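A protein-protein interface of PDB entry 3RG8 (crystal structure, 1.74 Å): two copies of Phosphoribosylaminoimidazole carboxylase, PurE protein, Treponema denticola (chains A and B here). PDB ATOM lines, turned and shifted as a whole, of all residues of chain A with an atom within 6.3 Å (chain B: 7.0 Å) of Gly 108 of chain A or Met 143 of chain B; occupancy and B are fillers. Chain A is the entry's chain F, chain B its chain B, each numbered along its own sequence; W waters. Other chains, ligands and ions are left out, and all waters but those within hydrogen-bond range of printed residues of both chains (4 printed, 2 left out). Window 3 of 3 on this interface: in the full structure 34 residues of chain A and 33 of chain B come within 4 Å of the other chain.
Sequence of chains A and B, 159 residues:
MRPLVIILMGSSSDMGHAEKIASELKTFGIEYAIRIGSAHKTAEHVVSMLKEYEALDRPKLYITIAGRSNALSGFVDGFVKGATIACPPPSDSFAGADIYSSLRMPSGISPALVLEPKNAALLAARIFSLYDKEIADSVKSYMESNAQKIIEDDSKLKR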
ATOM      1  N   ASP A  77       4.951  -8.419   1.094  1.00  0.00           N
ATOM      2  CA  ASP A  77       4.650  -9.220  -0.073  1.00  0.00           C
ATOM      3  C   ASP A  77       5.901  -9.533  -0.841  1.00  0.00           C
ATOM      4  O   ASP A  77       6.017 -10.596  -1.428  1.00  0.00           O
ATOM      5  CB  ASP A  77       3.711  -8.510  -1.028  1.00  0.00           C
ATOM      6  CG  ASP A  77       3.198  -9.452  -2.104  1.00  0.00           C
ATOM      7  OD1 ASP A  77       2.243 -10.261  -1.807  1.00  0.00           O
ATOM      8  OD2 ASP A  77       3.737  -9.366  -3.231  1.00  0.00           O
ATOM      9  N   GLY A  78       6.829  -8.593  -0.850  1.00  0.00           N
ATOM     10  CA  GLY A  78       8.095  -8.817  -1.541  1.00  0.00           C
ATOM     11  C   GLY A  78       9.033  -9.734  -0.729  1.00  0.00           C
ATOM     12  O   GLY A  78       9.994 -10.286  -1.269  1.00  0.00           O
ATOM     13  N   PHE A  79       8.785  -9.875   0.565  1.00  0.00           N
ATOM     14  CA  PHE A  79       9.654 -10.665   1.397  1.00  0.00           C
ATOM     15  C   PHE A  79       9.252 -12.148   1.457  1.00  0.00           C
ATOM     16  O   PHE A  79      10.118 -13.063   1.456  1.00  0.00           O
ATOM     17  CB  PHE A  79       9.708 -10.107   2.805  1.00  0.00           C
ATOM     18  CG  PHE A  79      10.792 -10.723   3.591  1.00  0.00           C
ATOM     19  CD1 PHE A  79      10.554 -11.848   4.348  1.00  0.00           C
ATOM     20  CD2 PHE A  79      12.101 -10.259   3.449  1.00  0.00           C
ATOM     21  CE1 PHE A  79      11.595 -12.458   5.027  1.00  0.00           C
ATOM     22  CE2 PHE A  79      13.144 -10.846   4.135  1.00  0.00           C
ATOM     23  CZ  PHE A  79      12.897 -11.950   4.920  1.00  0.00           C
ATOM     24  N   VAL A  80       7.949 -12.387   1.570  1.00  0.00           N
ATOM     25  CA  VAL A  80       7.434 -13.738   1.777  1.00  0.00           C
ATOM     26  C   VAL A  80       7.164 -14.404   0.431  1.00  0.00           C
ATOM     27  O   VAL A  80       7.033 -13.717  -0.581  1.00  0.00           O
ATOM     28  CB  VAL A  80       6.131 -13.767   2.635  1.00  0.00           C
ATOM     29  CG1 VAL A  80       6.356 -12.980   3.977  1.00  0.00           C
ATOM     30  CG2 VAL A  80       4.886 -13.239   1.846  1.00  0.00           C
ATOM     31  N   LYS A  81       7.085 -15.724   0.462  1.00  0.00           N
ATOM     32  CA  LYS A  81       6.980 -16.572  -0.738  1.00  0.00           C
ATOM     33  C   LYS A  81       5.536 -16.745  -1.157  1.00  0.00           C
ATOM     34  O   LYS A  81       5.209 -16.656  -2.338  1.00  0.00           O
ATOM     35  CB  LYS A  81       7.567 -17.990  -0.508  1.00  0.00           C
ATOM     36  CG  LYS A  81       8.831 -18.129   0.401  1.00  0.00           C
ATOM     37  CD  LYS A  81       8.883 -19.433   1.251  1.00  0.00           C
ATOM     38  CE  LYS A  81       7.601 -19.700   2.048  1.00  0.00           C
ATOM     39  NZ  LYS A  81       7.764 -20.777   3.065  1.00  0.00           N
ATOM     40  N   PRO A 106       4.749  -2.248  -7.850  1.00  0.00           N
ATOM     41  CA  PRO A 106       5.589  -2.494  -8.999  1.00  0.00           C
ATOM     42  C   PRO A 106       5.264  -3.851  -9.597  1.00  0.00           C
ATOM     43  O   PRO A 106       4.553  -4.649  -8.985  1.00  0.00           O
ATOM     44  CB  PRO A 106       6.986  -2.475  -8.418  1.00  0.00           C
ATOM     45  CG  PRO A 106       6.856  -3.008  -7.095  1.00  0.00           C
ATOM     46  CD  PRO A 106       5.495  -2.416  -6.588  1.00  0.00           C
ATOM     47  N   SER A 107       5.742  -4.078 -10.807  1.00  0.00           N
ATOM     48  CA  SER A 107       5.720  -5.413 -11.402  1.00  0.00           C
ATOM     49  C   SER A 107       6.465  -6.405 -10.453  1.00  0.00           C
ATOM     50  O   SER A 107       7.508  -6.069  -9.936  1.00  0.00           O
ATOM     51  CB  SER A 107       6.397  -5.335 -12.743  1.00  0.00           C
ATOM     52  OG  SER A 107       6.468  -6.614 -13.345  1.00  0.00           O
ATOM     53  N   GLY A 108       5.890  -7.572 -10.157  1.00  0.00           N
ATOM     54  CA  GLY A 108       6.502  -8.542  -9.202  1.00  0.00           C
ATOM     55  C   GLY A 108       6.125  -8.489  -7.710  1.00  0.00           C
ATOM     56  O   GLY A 108       6.702  -9.218  -6.889  1.00  0.00           O
ATOM     57  N   ILE A 109       5.177  -7.626  -7.354  1.00  0.00           N
ATOM     58  CA  ILE A 109       4.623  -7.519  -6.016  1.00  0.00           C
ATOM     59  C   ILE A 109       3.111  -7.667  -6.199  1.00  0.00           C
ATOM     60  O   ILE A 109       2.462  -6.878  -6.933  1.00  0.00           O
ATOM     61  CB  ILE A 109       5.045  -6.181  -5.324  1.00  0.00           C
ATOM     62  CG1 ILE A 109       6.570  -6.095  -5.168  1.00  0.00           C
ATOM     63  CG2 ILE A 109       4.398  -6.006  -3.963  1.00  0.00           C
ATOM     64  CD1 ILE A 109       7.178  -7.039  -4.109  1.00  0.00           C
ATOM     65  N   SER A 110       2.518  -8.657  -5.535  1.00  0.00           N
ATOM     66  CA  SER A 110       1.178  -9.045  -5.933  1.00  0.00           C
ATOM     67  C   SER A 110       0.211  -9.256  -4.769  1.00  0.00           C
ATOM     68  O   SER A 110      -0.545 -10.254  -4.764  1.00  0.00           O
ATOM     69  CB  SER A 110       1.234 -10.299  -6.805  1.00  0.00           C
ATOM     70  OG  SER A 110       1.621 -11.406  -6.038  1.00  0.00           O
ATOM     71  N   PHE B  28       4.706 -19.962 -15.216  1.00  0.00           N
ATOM     72  CA  PHE B  28       4.634 -20.612 -13.898  1.00  0.00           C
ATOM     73  C   PHE B  28       4.150 -22.097 -13.982  1.00  0.00           C
ATOM     74  O   PHE B  28       3.960 -22.750 -12.951  1.00  0.00           O
ATOM     75  CB  PHE B  28       3.701 -19.827 -12.942  1.00  0.00           C
ATOM     76  CG  PHE B  28       4.185 -18.440 -12.595  1.00  0.00           C
ATOM     77  CD1 PHE B  28       5.327 -18.248 -11.843  1.00  0.00           C
ATOM     78  CD2 PHE B  28       3.467 -17.320 -12.992  1.00  0.00           C
ATOM     79  CE1 PHE B  28       5.748 -16.965 -11.512  1.00  0.00           C
ATOM     80  CE2 PHE B  28       3.886 -16.061 -12.674  1.00  0.00           C
ATOM     81  CZ  PHE B  28       5.042 -15.868 -11.958  1.00  0.00           C
ATOM     82  N   GLU B 116      -2.074  -5.093 -12.281  1.00  0.00           N
ATOM     83  CA  GLU B 116      -1.181  -5.362 -13.403  1.00  0.00           C
ATOM     84  C   GLU B 116      -1.367  -6.823 -13.803  1.00  0.00           C
ATOM     85  O   GLU B 116      -1.416  -7.687 -12.934  1.00  0.00           O
ATOM     86  CB  GLU B 116       0.263  -5.128 -12.997  1.00  0.00           C
ATOM     87  CG  GLU B 116       0.566  -3.685 -12.537  1.00  0.00           C
ATOM     88  CD  GLU B 116       1.482  -2.978 -13.447  1.00  0.00           C
ATOM     89  OE1 GLU B 116       2.350  -3.662 -14.015  1.00  0.00           O
ATOM     90  OE2 GLU B 116       1.389  -1.734 -13.561  1.00  0.00           O
ATOM     91  N   LYS B 118       0.533  -9.161 -15.157  1.00  0.00           N
ATOM     92  CA  LYS B 118       1.521 -10.093 -14.638  1.00  0.00           C
ATOM     93  C   LYS B 118       1.429 -10.276 -13.121  1.00  0.00           C
ATOM     94  O   LYS B 118       1.732 -11.352 -12.617  1.00  0.00           O
ATOM     95  CB  LYS B 118       2.936  -9.713 -15.034  1.00  0.00           C
ATOM     96  CG  LYS B 118       3.185  -9.613 -16.513  1.00  0.00           C
ATOM     97  CD  LYS B 118       4.631  -9.242 -16.685  1.00  0.00           C
ATOM     98  CE  LYS B 118       5.030  -9.301 -18.084  1.00  0.00           C
ATOM     99  NZ  LYS B 118       6.517  -9.220 -18.165  1.00  0.00           N
ATOM    100  N   ASN B 119       0.975  -9.269 -12.365  1.00  0.00           N
ATOM    101  CA  ASN B 119       0.872  -9.480 -10.951  1.00  0.00           C
ATOM    102  C   ASN B 119      -0.376 -10.266 -10.624  1.00  0.00           C
ATOM    103  O   ASN B 119      -0.384 -11.057  -9.661  1.00  0.00           O
ATOM    104  CB  ASN B 119       0.869  -8.158 -10.175  1.00  0.00           C
ATOM    105  CG  ASN B 119       2.228  -7.470 -10.156  1.00  0.00           C
ATOM    106  OD1 ASN B 119       3.310  -8.081 -10.219  1.00  0.00           O
ATOM    107  ND2 ASN B 119       2.161  -6.139 -10.094  1.00  0.00           N
ATOM    108  N   LEU B 122       0.920 -13.661 -10.953  1.00  0.00           N
ATOM    109  CA  LEU B 122       1.838 -13.932  -9.846  1.00  0.00           C
ATOM    110  C   LEU B 122       0.975 -14.230  -8.622  1.00  0.00           C
ATOM    111  O   LEU B 122       1.245 -15.196  -7.915  1.00  0.00           O
ATOM    112  CB  LEU B 122       2.753 -12.752  -9.550  1.00  0.00           C
ATOM    113  CG  LEU B 122       3.736 -12.900  -8.382  1.00  0.00           C
ATOM    114  CD1 LEU B 122       4.566 -14.185  -8.579  1.00  0.00           C
ATOM    115  CD2 LEU B 122       4.634 -11.683  -8.252  1.00  0.00           C
ATOM    116  N   ARG B 126       0.957 -17.718  -6.470  1.00  0.00           N
ATOM    117  CA  ARG B 126       1.282 -17.701  -5.051  1.00  0.00           C
ATOM    118  C   ARG B 126       0.084 -18.257  -4.226  1.00  0.00           C
ATOM    119  O   ARG B 126       0.256 -18.825  -3.124  1.00  0.00           O
ATOM    120  CB  ARG B 126       1.730 -16.259  -4.646  1.00  0.00           C
ATOM    121  CG  ARG B 126       3.095 -15.847  -5.319  1.00  0.00           C
ATOM    122  CD  ARG B 126       3.440 -14.459  -5.075  1.00  0.00           C
ATOM    123  NE  ARG B 126       3.876 -14.204  -3.703  1.00  0.00           N
ATOM    124  CZ  ARG B 126       4.231 -13.011  -3.248  1.00  0.00           C
ATOM    125  NH1 ARG B 126       4.122 -11.918  -4.008  1.00  0.00           N
ATOM    126  NH2 ARG B 126       4.601 -12.897  -1.981  1.00  0.00           N
ATOM    127  N   SER B 138       8.573 -22.420  -8.692  1.00  0.00           N
ATOM    128  CA  SER B 138       8.593 -21.518  -9.839  1.00  0.00           C
ATOM    129  C   SER B 138       8.516 -20.049  -9.422  1.00  0.00           C
ATOM    130  O   SER B 138       9.289 -19.230  -9.904  1.00  0.00           O
ATOM    131  CB  SER B 138       7.483 -21.810 -10.811  1.00  0.00           C
ATOM    132  OG  SER B 138       7.764 -21.175 -12.053  1.00  0.00           O
ATOM    133  N   VAL B 139       7.565 -19.747  -8.551  1.00  0.00           N
ATOM    134  CA  VAL B 139       7.448 -18.417  -7.941  1.00  0.00           C
ATOM    135  C   VAL B 139       8.747 -18.021  -7.244  1.00  0.00           C
ATOM    136  O   VAL B 139       9.171 -16.901  -7.373  1.00  0.00           O
ATOM    137  CB  VAL B 139       6.328 -18.385  -6.884  1.00  0.00           C
ATOM    138  CG1 VAL B 139       6.445 -17.147  -6.012  1.00  0.00           C
ATOM    139  CG2 VAL B 139       4.910 -18.521  -7.545  1.00  0.00           C
ATOM    140  N   LYS B 140       9.334 -18.913  -6.449  1.00  0.00           N
ATOM    141  CA  LYS B 140      10.630 -18.632  -5.794  1.00  0.00           C
ATOM    142  C   LYS B 140      11.673 -18.158  -6.788  1.00  0.00           C
ATOM    143  O   LYS B 140      12.241 -17.067  -6.652  1.00  0.00           O
ATOM    144  CB  LYS B 140      11.155 -19.870  -5.053  1.00  0.00           C
ATOM    145  CG  LYS B 140      12.237 -19.613  -4.025  1.00  0.00           C
ATOM    146  CD  LYS B 140      12.556 -20.936  -3.286  1.00  0.00           C
ATOM    147  CE  LYS B 140      13.873 -20.917  -2.559  1.00  0.00           C
ATOM    148  NZ  LYS B 140      14.233 -22.298  -2.061  1.00  0.00           N
ATOM    149  N   SER B 141      11.907 -18.959  -7.815  1.00  0.00           N
ATOM    150  CA  SER B 141      12.866 -18.607  -8.815  1.00  0.00           C
ATOM    151  C   SER B 141      12.575 -17.229  -9.439  1.00  0.00           C
ATOM    152  O   SER B 141      13.495 -16.448  -9.637  1.00  0.00           O
ATOM    153  CB  SER B 141      12.903 -19.692  -9.893  1.00  0.00           C
ATOM    154  OG  SER B 141      13.580 -19.218 -11.025  1.00  0.00           O
ATOM    155  N   TYR B 142      11.314 -17.002  -9.775  1.00  0.00           N
ATOM    156  CA  TYR B 142      10.861 -15.758 -10.426  1.00  0.00           C
ATOM    157  C   TYR B 142      11.160 -14.545  -9.556  1.00  0.00           C
ATOM    158  O   TYR B 142      11.792 -13.592 -10.017  1.00  0.00           O
ATOM    159  CB  TYR B 142       9.366 -15.819 -10.770  1.00  0.00           C
ATOM    160  CG  TYR B 142       8.907 -14.569 -11.506  1.00  0.00           C
ATOM    161  CD1 TYR B 142       9.440 -14.252 -12.754  1.00  0.00           C
ATOM    162  CD2 TYR B 142       8.015 -13.674 -10.924  1.00  0.00           C
ATOM    163  CE1 TYR B 142       9.071 -13.104 -13.432  1.00  0.00           C
ATOM    164  CE2 TYR B 142       7.626 -12.504 -11.599  1.00  0.00           C
ATOM    165  CZ  TYR B 142       8.181 -12.229 -12.859  1.00  0.00           C
ATOM    166  OH  TYR B 142       7.836 -11.091 -13.579  1.00  0.00           O
ATOM    167  N   MET B 143      10.738 -14.591  -8.298  1.00  0.00           N
ATOM    168  CA  MET B 143      10.892 -13.421  -7.400  1.00  0.00           C
ATOM    169  C   MET B 143      12.329 -13.172  -7.004  1.00  0.00           C
ATOM    170  O   MET B 143      12.757 -12.025  -6.910  1.00  0.00           O
ATOM    171  CB  MET B 143       9.978 -13.516  -6.163  1.00  0.00           C
ATOM    172  CG  MET B 143       8.549 -13.430  -6.532  1.00  0.00           C
ATOM    173  SD  MET B 143       7.368 -13.544  -5.157  1.00  0.00           S
ATOM    174  CE  MET B 143       7.348 -11.848  -4.560  1.00  0.00           C
ATOM    175  N   GLU B 144      13.090 -14.241  -6.766  1.00  0.00           N
ATOM    176  CA  GLU B 144      14.524 -14.107  -6.505  1.00  0.00           C
ATOM    177  C   GLU B 144      15.285 -13.532  -7.684  1.00  0.00           C
ATOM    178  O   GLU B 144      16.221 -12.747  -7.501  1.00  0.00           O
ATOM    179  CB  GLU B 144      15.121 -15.442  -6.099  1.00  0.00           C
ATOM    180  CG  GLU B 144      14.734 -15.880  -4.707  1.00  0.00           C
ATOM    181  CD  GLU B 144      15.476 -17.163  -4.309  1.00  0.00           C
ATOM    182  OE1 GLU B 144      16.425 -17.554  -5.027  1.00  0.00           O
ATOM    183  OE2 GLU B 144      15.122 -17.781  -3.294  1.00  0.00           O
ATOM    184  N   SER B 145      14.882 -13.884  -8.902  1.00  0.00           N
ATOM    185  CA  SER B 145      15.573 -13.360 -10.092  1.00  0.00           C
ATOM    186  C   SER B 145      15.396 -11.823 -10.200  1.00  0.00           C
ATOM    187  O   SER B 145      16.387 -11.084 -10.371  1.00  0.00           O
ATOM    188  CB  SER B 145      15.055 -14.067 -11.350  1.00  0.00           C
ATOM    189  OG  SER B 145      15.647 -13.512 -12.504  1.00  0.00           O
ATOM    190  N   ASN B 146      14.140 -11.394 -10.101  1.00  0.00           N
ATOM    191  CA  ASN B 146      13.727  -9.982 -10.087  1.00  0.00           C
ATOM    192  C   ASN B 146      14.534  -9.180  -9.081  1.00  0.00           C
ATOM    193  O   ASN B 146      14.999  -8.076  -9.369  1.00  0.00           O
ATOM    194  CB  ASN B 146      12.249  -9.880  -9.675  1.00  0.00           C
ATOM    195  CG  ASN B 146      11.282 -10.292 -10.777  1.00  0.00           C
ATOM    196  OD1 ASN B 146      11.680 -10.699 -11.857  1.00  0.00           O
ATOM    197  ND2 ASN B 146       9.991 -10.185 -10.495  1.00  0.00           N
ATOM    198  N   ALA B 147      14.679  -9.730  -7.881  1.00  0.00           N
ATOM    199  CA  ALA B 147      15.460  -9.076  -6.854  1.00  0.00           C
ATOM    200  C   ALA B 147      16.914  -9.054  -7.273  1.00  0.00           C
ATOM    201  O   ALA B 147      17.562  -7.997  -7.187  1.00  0.00           O
ATOM    202  CB  ALA B 147      15.292  -9.769  -5.516  1.00  0.00           C
ATOM    203  N   GLN B 148      17.455 -10.190  -7.759  1.00  0.00           N
ATOM    204  CA  GLN B 148      18.882 -10.222  -8.138  1.00  0.00           C
ATOM    205  C   GLN B 148      19.177  -9.191  -9.249  1.00  0.00           C
ATOM    206  O   GLN B 148      20.225  -8.570  -9.245  1.00  0.00           O
ATOM    207  CB  GLN B 148      19.419 -11.656  -8.520  1.00  0.00           C
ATOM    208  CG  GLN B 148      21.025 -11.698  -8.644  1.00  0.00           C
ATOM    209  CD  GLN B 148      21.758 -13.070  -9.005  1.00  0.00           C
ATOM    210  OE1 GLN B 148      21.283 -14.178  -8.725  1.00  0.00           O
ATOM    211  NE2 GLN B 148      22.946 -12.947  -9.603  1.00  0.00           N
HETATM  212  O   HOH W   1       9.265  -9.983  -7.682  1.00  0.00           O
HETATM  213  O   HOH W   2       3.688  -5.995 -14.299  1.00  0.00           O
HETATM  214  O   HOH W   3       4.798  -9.822 -11.922  1.00  0.00           O
HETATM  215  O   HOH W   4      -0.236  -5.944  -7.745  1.00  0.00           O
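Water W2 bridges the side-chain carboxylate (OE1) of Glu 116 of chain B and the side-chain hydroxyl (OG) of Ser 107 of chain A. Water W1 bridges the backbone carbonyl oxygen (O) of Gly 108 of chain A (2.8 Å) and the side-chain amide nitrogen (ND2) of Asn 146 of chain B (2.9 Å). Water W3 lies within hydrogen-bond range of OD1 of Asn 119 of chain B (2.9 Å), N of Gly 108 of chain A (3.1 Å) and O of Lys 118 of chain B (3.5 Å). Water W4 lies within hydrogen-bond range of O of Ile 109 of chain A and ND2 of Asn 119 of chain B.
No position is printed for both chains. Of the 14 pairs that touch across the chains among the printed residues, none has its exchanged pair printed and touching as well.
Gly 108 of chain A touches just these residues of chain B: Asn 119 (2.6 Å), Leu 122 (3.5 Å) and Met 143 (3.6 Å). Of chain A, only Asp 77 and Gly 108 come within 4 Å of Met 143 of chain B. Of the printed residues of chain A, Asn 119 of chain B touches Pro 106 (3.0 Å), Ser 107 (3.6 Å), Gly 108 (2.6 Å), Ile 109 (3.3 Å) and Ser 110 (3.4 Å). Printed residues of chain B within 4 Å of Pro 106 of chain A: Asn 119. The nearest residue of chain B that does not touch Gly 108 of chain A is Asn 146 of chain B (4.1 Å). The nearest residue of chain A that does not touch Met 143 of chain B is Gly 78 of chain A (4.3 Å).
Printed residues of chain B that touch a printed residue of chain A: Asn 119, Leu 122, Arg 126, Val 139 and Met 143. Hydrophobic or aromatic side chains of chain B that line the printed part of chain A: Leu 122, Val 139 and Met 143. Along chain A the printed residues that touch a printed residue of chain B span positions 77 to 110. Among the printed residues, 14 pairs touch across the chains. Among the printed residues, Asp or Glu carboxylates within 4 Å of a Lys or Arg side-chain nitrogen of the other chain: Asp 77 of chain A with Arg 126 of chain B (2.7 Å).
ND2 of Asn 119 of chain B sits at hydrogen-bond distance from O of Pro 106 of chain A (3.0 Å). N of Gly 108 of chain A lies within hydrogen-bond range of OD1 of Asn 119 of chain B (2.6 Å). The side-chain amide nitrogen (ND2) of Asn 119 of chain B lies within hydrogen-bond range of the backbone carbonyl oxygen (O) of Ile 109 of chain A (3.3 Å). The side-chain carboxylate (OD2) of Asp 77 of chain A is in salt-bridge range of the guanidinium group (NH1) of Arg 126 of chain B, at 2.7 Å. The backbone carbonyl oxygen (O) of Val 80 of chain A is in hydrogen-bond range of the guanidinium group (NH2) of Arg 126 of chain B, 2.9 Å away. O of Lys 81 of chain A sits at hydrogen-bond distance from NE of Arg 126 of chain B (3.1 Å). The guanidinium group (NH1) of Arg 126 of chain B lies within hydrogen-bond range of the side-chain hydroxyl (OG) of Ser 110 of chain A.
Among the printed residues, pairs that only touch across the chains: Ser 110 of chain A with Asn 119 of chain B, Ser 110 of chain A with Leu 122 of chain B, Gly 108 of chain A with Leu 122 of chain B, Gly 108 of chain A with Met 143 of chain B, Ser 107 of chain A with Asn 119 of chain B, Asp 77 of chain A with Met 143 of chain B and Lys 81 of chain A with Val 139 of chain B.
N of Ser 110 of chain A is in hydrogen-bond range of OD2 of Asp 77 of chain A (2.7 Å).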
